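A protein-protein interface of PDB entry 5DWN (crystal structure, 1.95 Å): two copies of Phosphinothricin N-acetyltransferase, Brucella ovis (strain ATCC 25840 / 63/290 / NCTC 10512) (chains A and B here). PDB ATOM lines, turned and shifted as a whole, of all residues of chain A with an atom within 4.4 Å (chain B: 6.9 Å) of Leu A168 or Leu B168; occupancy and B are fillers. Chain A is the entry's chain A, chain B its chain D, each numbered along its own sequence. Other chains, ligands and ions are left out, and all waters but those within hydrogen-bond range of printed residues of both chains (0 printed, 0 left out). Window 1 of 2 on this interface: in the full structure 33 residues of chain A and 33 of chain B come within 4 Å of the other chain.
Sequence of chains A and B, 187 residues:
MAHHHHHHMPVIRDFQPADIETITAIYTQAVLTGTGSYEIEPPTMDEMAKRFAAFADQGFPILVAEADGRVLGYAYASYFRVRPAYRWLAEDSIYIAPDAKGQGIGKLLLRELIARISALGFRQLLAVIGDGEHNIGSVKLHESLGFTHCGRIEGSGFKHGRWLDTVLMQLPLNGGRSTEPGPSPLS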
ATOM      1  N   ALA A 127      31.524  19.316 -15.764  1.00  0.00           N
ATOM      2  CA  ALA A 127      30.394  19.609 -14.890  1.00  0.00           C
ATOM      3  C   ALA A 127      29.262  18.657 -15.244  1.00  0.00           C
ATOM      4  O   ALA A 127      28.816  18.627 -16.393  1.00  0.00           O
ATOM      5  CB  ALA A 127      29.932  21.059 -15.043  1.00  0.00           C
ATOM      6  N   VAL A 128      28.794  17.895 -14.266  1.00  0.00           N
ATOM      7  CA  VAL A 128      27.649  17.012 -14.448  1.00  0.00           C
ATOM      8  C   VAL A 128      26.495  17.655 -13.694  1.00  0.00           C
ATOM      9  O   VAL A 128      26.418  17.557 -12.465  1.00  0.00           O
ATOM     10  CB  VAL A 128      27.933  15.591 -13.953  1.00  0.00           C
ATOM     11  CG1 VAL A 128      26.716  14.693 -14.221  1.00  0.00           C
ATOM     12  CG2 VAL A 128      29.157  15.038 -14.668  1.00  0.00           C
ATOM     13  N   THR A 148      31.841  24.792 -21.889  1.00  0.00           N
ATOM     14  CA  THR A 148      30.983  24.675 -23.063  1.00  0.00           C
ATOM     15  C   THR A 148      30.093  23.449 -22.928  1.00  0.00           C
ATOM     16  O   THR A 148      30.472  22.464 -22.292  1.00  0.00           O
ATOM     17  CB  THR A 148      31.810  24.584 -24.357  1.00  0.00           C
ATOM     18  OG1 THR A 148      32.652  23.431 -24.288  1.00  0.00           O
ATOM     19  CG2 THR A 148      32.702  25.813 -24.511  1.00  0.00           C
ATOM     20  N   HIS A 149      28.905  23.505 -23.537  1.00  0.00           N
ATOM     21  CA  HIS A 149      27.982  22.378 -23.444  1.00  0.00           C
ATOM     22  C   HIS A 149      28.555  21.187 -24.193  1.00  0.00           C
ATOM     23  O   HIS A 149      29.078  21.336 -25.297  1.00  0.00           O
ATOM     24  CB  HIS A 149      26.610  22.759 -24.009  1.00  0.00           C
ATOM     25  CG  HIS A 149      25.851  23.680 -23.112  1.00  0.00           C
ATOM     26  ND1 HIS A 149      24.962  23.225 -22.161  1.00  0.00           N
ATOM     27  CD2 HIS A 149      25.908  25.026 -22.963  1.00  0.00           C
ATOM     28  CE1 HIS A 149      24.485  24.254 -21.482  1.00  0.00           C
ATOM     29  NE2 HIS A 149      25.038  25.358 -21.954  1.00  0.00           N
ATOM     30  N   CYS A 150      28.480  20.003 -23.589  1.00  0.00           N
ATOM     31  CA  CYS A 150      28.974  18.817 -24.278  1.00  0.00           C
ATOM     32  C   CYS A 150      28.025  17.635 -24.139  1.00  0.00           C
ATOM     33  O   CYS A 150      28.427  16.493 -24.394  1.00  0.00           O
ATOM     34  CB  CYS A 150      30.382  18.436 -23.800  1.00  0.00           C
ATOM     35  SG  CYS A 150      30.565  18.022 -22.042  1.00  0.00           S
ATOM     36  N   GLY A 151      26.781  17.870 -23.754  1.00  0.00           N
ATOM     37  CA  GLY A 151      25.811  16.794 -23.812  1.00  0.00           C
ATOM     38  C   GLY A 151      24.665  17.010 -22.859  1.00  0.00           C
ATOM     39  O   GLY A 151      24.663  17.927 -22.045  1.00  0.00           O
ATOM     40  N   THR A 166      20.217  15.509 -17.187  1.00  0.00           N
ATOM     41  CA  THR A 166      21.577  15.820 -16.784  1.00  0.00           C
ATOM     42  C   THR A 166      22.249  16.611 -17.895  1.00  0.00           C
ATOM     43  O   THR A 166      22.322  16.141 -19.033  1.00  0.00           O
ATOM     44  CB  THR A 166      22.366  14.546 -16.518  1.00  0.00           C
ATOM     45  OG1 THR A 166      21.821  13.875 -15.375  1.00  0.00           O
ATOM     46  CG2 THR A 166      23.837  14.901 -16.273  1.00  0.00           C
ATOM     47  N   VAL A 167      22.746  17.795 -17.571  1.00  0.00           N
ATOM     48  CA  VAL A 167      23.444  18.629 -18.543  1.00  0.00           C
ATOM     49  C   VAL A 167      24.939  18.479 -18.297  1.00  0.00           C
ATOM     50  O   VAL A 167      25.404  18.619 -17.156  1.00  0.00           O
ATOM     51  CB  VAL A 167      22.975  20.094 -18.438  1.00  0.00           C
ATOM     52  CG1 VAL A 167      23.977  21.070 -19.093  1.00  0.00           C
ATOM     53  CG2 VAL A 167      21.573  20.244 -19.070  1.00  0.00           C
ATOM     54  N   LEU A 168      25.694  18.162 -19.352  1.00  0.00           N
ATOM     55  CA  LEU A 168      27.143  18.021 -19.237  1.00  0.00           C
ATOM     56  C   LEU A 168      27.828  19.208 -19.896  1.00  0.00           C
ATOM     57  O   LEU A 168      27.458  19.616 -21.007  1.00  0.00           O
ATOM     58  CB  LEU A 168      27.647  16.730 -19.896  1.00  0.00           C
ATOM     59  CG  LEU A 168      26.960  15.475 -19.383  1.00  0.00           C
ATOM     60  CD1 LEU A 168      27.305  14.356 -20.329  1.00  0.00           C
ATOM     61  CD2 LEU A 168      27.435  15.149 -17.982  1.00  0.00           C
ATOM     62  N   MET A 169      28.835  19.742 -19.214  1.00  0.00           N
ATOM     63  CA  MET A 169      29.640  20.841 -19.730  1.00  0.00           C
ATOM     64  C   MET A 169      31.100  20.563 -19.409  1.00  0.00           C
ATOM     65  O   MET A 169      31.408  19.879 -18.430  1.00  0.00           O
ATOM     66  CB  MET A 169      29.209  22.179 -19.121  1.00  0.00           C
ATOM     67  CG  MET A 169      27.715  22.426 -19.235  1.00  0.00           C
ATOM     68  SD  MET A 169      27.255  24.025 -18.591  1.00  0.00           S
ATOM     69  CE  MET A 169      28.037  25.145 -19.762  1.00  0.00           C
ATOM     70  N   PHE B  80      24.875   3.765 -14.351  1.00  0.00           N
ATOM     71  CA  PHE B  80      25.743   4.870 -14.748  1.00  0.00           C
ATOM     72  C   PHE B  80      26.337   5.549 -13.519  1.00  0.00           C
ATOM     73  O   PHE B  80      27.560   5.685 -13.403  1.00  0.00           O
ATOM     74  CB  PHE B  80      24.980   5.873 -15.611  1.00  0.00           C
ATOM     75  CG  PHE B  80      25.688   7.205 -15.757  1.00  0.00           C
ATOM     76  CD1 PHE B  80      26.885   7.291 -16.449  1.00  0.00           C
ATOM     77  CD2 PHE B  80      25.155   8.357 -15.190  1.00  0.00           C
ATOM     78  CE1 PHE B  80      27.547   8.504 -16.585  1.00  0.00           C
ATOM     79  CE2 PHE B  80      25.808   9.582 -15.320  1.00  0.00           C
ATOM     80  CZ  PHE B  80      27.006   9.650 -16.019  1.00  0.00           C
ATOM     81  N   LEU B 126      22.047   3.850 -21.287  1.00  0.00           N
ATOM     82  CA  LEU B 126      23.116   4.757 -21.684  1.00  0.00           C
ATOM     83  C   LEU B 126      24.305   3.964 -22.205  1.00  0.00           C
ATOM     84  O   LEU B 126      24.762   3.022 -21.550  1.00  0.00           O
ATOM     85  CB  LEU B 126      23.553   5.620 -20.493  1.00  0.00           C
ATOM     86  CG  LEU B 126      24.609   6.694 -20.780  1.00  0.00           C
ATOM     87  CD1 LEU B 126      24.008   7.800 -21.642  1.00  0.00           C
ATOM     88  CD2 LEU B 126      25.164   7.253 -19.456  1.00  0.00           C
ATOM     89  N   ALA B 127      24.804   4.338 -23.380  1.00  0.00           N
ATOM     90  CA  ALA B 127      26.080   3.842 -23.875  1.00  0.00           C
ATOM     91  C   ALA B 127      27.141   4.915 -23.655  1.00  0.00           C
ATOM     92  O   ALA B 127      27.026   6.029 -24.175  1.00  0.00           O
ATOM     93  CB  ALA B 127      26.000   3.468 -25.358  1.00  0.00           C
ATOM     94  N   VAL B 128      28.163   4.578 -22.882  1.00  0.00           N
ATOM     95  CA  VAL B 128      29.314   5.445 -22.668  1.00  0.00           C
ATOM     96  C   VAL B 128      30.426   4.866 -23.537  1.00  0.00           C
ATOM     97  O   VAL B 128      31.094   3.903 -23.145  1.00  0.00           O
ATOM     98  CB  VAL B 128      29.702   5.504 -21.189  1.00  0.00           C
ATOM     99  CG1 VAL B 128      30.870   6.465 -20.978  1.00  0.00           C
ATOM    100  CG2 VAL B 128      28.480   5.918 -20.343  1.00  0.00           C
ATOM    101  N   ILE B 129      30.603   5.424 -24.733  1.00  0.00           N
ATOM    102  CA  ILE B 129      31.430   4.811 -25.768  1.00  0.00           C
ATOM    103  C   ILE B 129      32.815   5.440 -25.728  1.00  0.00           C
ATOM    104  O   ILE B 129      32.996   6.602 -26.110  1.00  0.00           O
ATOM    105  CB  ILE B 129      30.791   4.942 -27.158  1.00  0.00           C
ATOM    106  CG1 ILE B 129      29.392   4.321 -27.152  1.00  0.00           C
ATOM    107  CG2 ILE B 129      31.675   4.282 -28.216  1.00  0.00           C
ATOM    108  CD1 ILE B 129      28.654   4.440 -28.469  1.00  0.00           C
ATOM    109  N   THR B 148      20.163   7.136 -29.562  1.00  0.00           N
ATOM    110  CA  THR B 148      20.385   8.457 -30.138  1.00  0.00           C
ATOM    111  C   THR B 148      21.577   9.126 -29.461  1.00  0.00           C
ATOM    112  O   THR B 148      21.899   8.837 -28.307  1.00  0.00           O
ATOM    113  CB  THR B 148      19.147   9.353 -30.000  1.00  0.00           C
ATOM    114  OG1 THR B 148      18.906   9.632 -28.616  1.00  0.00           O
ATOM    115  CG2 THR B 148      17.914   8.671 -30.585  1.00  0.00           C
ATOM    116  N   HIS B 149      22.237  10.018 -30.196  1.00  0.00           N
ATOM    117  CA  HIS B 149      23.397  10.717 -29.659  1.00  0.00           C
ATOM    118  C   HIS B 149      22.956  11.748 -28.626  1.00  0.00           C
ATOM    119  O   HIS B 149      22.035  12.535 -28.876  1.00  0.00           O
ATOM    120  CB  HIS B 149      24.162  11.405 -30.790  1.00  0.00           C
ATOM    121  CG  HIS B 149      24.923  10.458 -31.665  1.00  0.00           C
ATOM    122  ND1 HIS B 149      26.162   9.962 -31.320  1.00  0.00           N
ATOM    123  CD2 HIS B 149      24.617   9.908 -32.867  1.00  0.00           C
ATOM    124  CE1 HIS B 149      26.592   9.154 -32.275  1.00  0.00           C
ATOM    125  NE2 HIS B 149      25.672   9.104 -33.225  1.00  0.00           N
ATOM    126  N   CYS B 150      23.605  11.744 -27.458  1.00  0.00           N
ATOM    127  CA  CYS B 150      23.240  12.686 -26.408  1.00  0.00           C
ATOM    128  C   CYS B 150      24.458  13.365 -25.777  1.00  0.00           C
ATOM    129  O   CYS B 150      24.344  13.954 -24.698  1.00  0.00           O
ATOM    130  CB  CYS B 150      22.379  11.996 -25.340  1.00  0.00           C
ATOM    131  SG  CYS B 150      23.170  10.621 -24.449  1.00  0.00           S
ATOM    132  N   GLY B 151      25.612  13.330 -26.421  1.00  0.00           N
ATOM    133  CA  GLY B 151      26.725  14.107 -25.914  1.00  0.00           C
ATOM    134  C   GLY B 151      28.056  13.514 -26.307  1.00  0.00           C
ATOM    135  O   GLY B 151      28.154  12.387 -26.798  1.00  0.00           O
ATOM    136  N   ARG B 152      29.096  14.311 -26.077  1.00  0.00           N
ATOM    137  CA  ARG B 152      30.445  13.896 -26.434  1.00  0.00           C
ATOM    138  C   ARG B 152      31.402  14.646 -25.521  1.00  0.00           C
ATOM    139  O   ARG B 152      31.496  15.874 -25.611  1.00  0.00           O
ATOM    140  CB  ARG B 152      30.709  14.186 -27.917  1.00  0.00           C
ATOM    141  CG  ARG B 152      32.128  14.028 -28.383  1.00  0.00           C
ATOM    142  CD  ARG B 152      32.162  14.033 -29.907  1.00  0.00           C
ATOM    143  NE  ARG B 152      33.443  13.565 -30.395  1.00  0.00           N
ATOM    144  CZ  ARG B 152      33.602  12.805 -31.470  1.00  0.00           C
ATOM    145  NH1 ARG B 152      32.551  12.414 -32.184  1.00  0.00           N
ATOM    146  NH2 ARG B 152      34.819  12.438 -31.830  1.00  0.00           N
ATOM    147  N   ILE B 153      32.077  13.930 -24.624  1.00  0.00           N
ATOM    148  CA  ILE B 153      33.072  14.552 -23.759  1.00  0.00           C
ATOM    149  C   ILE B 153      34.411  14.483 -24.484  1.00  0.00           C
ATOM    150  O   ILE B 153      35.016  13.412 -24.576  1.00  0.00           O
ATOM    151  CB  ILE B 153      33.150  13.874 -22.385  1.00  0.00           C
ATOM    152  CG1 ILE B 153      31.775  13.811 -21.717  1.00  0.00           C
ATOM    153  CG2 ILE B 153      34.160  14.626 -21.486  1.00  0.00           C
ATOM    154  CD1 ILE B 153      31.760  12.958 -20.441  1.00  0.00           C
ATOM    155  N   THR B 166      34.724  10.581 -25.422  1.00  0.00           N
ATOM    156  CA  THR B 166      33.650   9.713 -24.967  1.00  0.00           C
ATOM    157  C   THR B 166      32.374  10.125 -25.680  1.00  0.00           C
ATOM    158  O   THR B 166      31.930  11.267 -25.545  1.00  0.00           O
ATOM    159  CB  THR B 166      33.462   9.806 -23.455  1.00  0.00           C
ATOM    160  OG1 THR B 166      34.667   9.391 -22.799  1.00  0.00           O
ATOM    161  CG2 THR B 166      32.310   8.912 -23.032  1.00  0.00           C
ATOM    162  N   VAL B 167      31.801   9.211 -26.449  1.00  0.00           N
ATOM    163  CA  VAL B 167      30.536   9.441 -27.134  1.00  0.00           C
ATOM    164  C   VAL B 167      29.424   8.846 -26.283  1.00  0.00           C
ATOM    165  O   VAL B 167      29.458   7.657 -25.941  1.00  0.00           O
ATOM    166  CB  VAL B 167      30.544   8.835 -28.543  1.00  0.00           C
ATOM    167  CG1 VAL B 167      29.139   8.857 -29.139  1.00  0.00           C
ATOM    168  CG2 VAL B 167      31.501   9.613 -29.425  1.00  0.00           C
ATOM    169  N   LEU B 168      28.440   9.667 -25.944  1.00  0.00           N
ATOM    170  CA  LEU B 168      27.302   9.230 -25.156  1.00  0.00           C
ATOM    171  C   LEU B 168      26.087   9.059 -26.054  1.00  0.00           C
ATOM    172  O   LEU B 168      25.825   9.882 -26.940  1.00  0.00           O
ATOM    173  CB  LEU B 168      26.999  10.235 -24.047  1.00  0.00           C
ATOM    174  CG  LEU B 168      28.215  10.496 -23.156  1.00  0.00           C
ATOM    175  CD1 LEU B 168      28.099  11.891 -22.584  1.00  0.00           C
ATOM    176  CD2 LEU B 168      28.270   9.494 -22.052  1.00  0.00           C
ATOM    177  N   MET B 169      25.367   7.965 -25.835  1.00  0.00           N
ATOM    178  CA  MET B 169      24.162   7.644 -26.575  1.00  0.00           C
ATOM    179  C   MET B 169      23.171   7.047 -25.590  1.00  0.00           C
ATOM    180  O   MET B 169      23.567   6.405 -24.615  1.00  0.00           O
ATOM    181  CB  MET B 169      24.440   6.651 -27.717  1.00  0.00           C
ATOM    182  CG  MET B 169      25.500   7.115 -28.709  1.00  0.00           C
ATOM    183  SD  MET B 169      25.609   6.027 -30.136  1.00  0.00           S
ATOM    184  CE  MET B 169      24.115   6.471 -31.033  1.00  0.00           C
ATOM    185  N   GLN B 170      21.882   7.260 -25.841  1.00  0.00           N
ATOM    186  CA  GLN B 170      20.880   6.749 -24.917  1.00  0.00           C
ATOM    187  C   GLN B 170      19.691   6.187 -25.678  1.00  0.00           C
ATOM    188  O   GLN B 170      19.417   6.558 -26.820  1.00  0.00           O
ATOM    189  CB  GLN B 170      20.418   7.818 -23.916  1.00  0.00           C
ATOM    190  CG  GLN B 170      19.581   8.943 -24.493  1.00  0.00           C
ATOM    191  CD  GLN B 170      19.176   9.941 -23.416  1.00  0.00           C
ATOM    192  OE1 GLN B 170      19.438  11.138 -23.528  1.00  0.00           O
ATOM    193  NE2 GLN B 170      18.548   9.444 -22.361  1.00  0.00           N
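O of Cys A150 lies within hydrogen-bond range of N of Arg B152 (2.8 Å).
Of the printed residues of chain B, Cys A150 touches Gly B151 (3.3 Å) and Arg B152 (2.8 Å). Of the printed residues of chain B, Gly A151 touches Cys B150 and Gly B151. Of chain B, only Leu B168 (3.4 Å) comes within 4 Å of Leu A168. Of the printed residues of chain A, Cys B150 touches Gly A151 (3.3 Å). Of the printed residues of chain A, Gly B151 touches Cys A150 (3.3 Å) and Gly A151 (3.5 Å). Printed residues of chain A within 4 Å of Arg B152: Cys A150 (2.8 Å). Of chain A, only Leu A168 (3.4 Å) comes within 4 Å of Leu B168. The nearest residue of chain B that does not touch Leu A168 is Ile B153 (4.7 Å). The nearest printed residue of chain A that does not touch Leu B168 is Cys A150 (5.0 Å). The nearest printed residue of chain B that does not touch Cys A150 is Ile B153 (4.4 Å).
Cys A150 touches Gly B151, and with the chains exchanged Gly A151 touches Cys B150. Gly B151 touches its own counterpart, Gly A151. Leu A168 touches its own counterpart, Leu B168.
Cys A150 touches Gly B151 (O to CA, 3.3 Å). Gly A151 touches Cys B150 (CA to O, 3.3 Å). Gly B151 touches Gly A151. Leu A168 touches Leu B168.
The backbone NH of Cys A150 sits at hydrogen-bond distance from the backbone carbonyl oxygen of Leu A168 (2.8 Å). The backbone NH (N) of Met A169 sits close to the side-chain sulfur (SG) of Cys A150, 3.7 Å away. The backbone carbonyl oxygen (O) of Gly A151 lies within hydrogen-bond range of the backbone NH (N) of Leu A168, at 2.9 Å. The backbone NH (N) of Cys B150 lies within hydrogen-bond range of the backbone carbonyl oxygen (O) of Leu B168 (2.9 Å). SG of Cys B150 sits at hydrogen-bond distance from N of Met B169, at 3.7 Å. The backbone carbonyl oxygen (O) of Gly B151 is in hydrogen-bond range of the backbone NH (N) of Leu B168 (2.9 Å).
Of the 16 printed residues of chain B, 4 touch a printed residue of chain A. Printed residues of chain B that touch a printed residue of chain A: Cys B150, Gly B151, Arg B152 and Leu B168. Hydrophobic or aromatic side chains of chain B that line the printed part of chain A: Leu B168. Hydrophobic or aromatic side chains of chain A within 4 Å of the printed part of chain B: Leu A168. Among the printed residues, 5 pairs touch across the chains.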
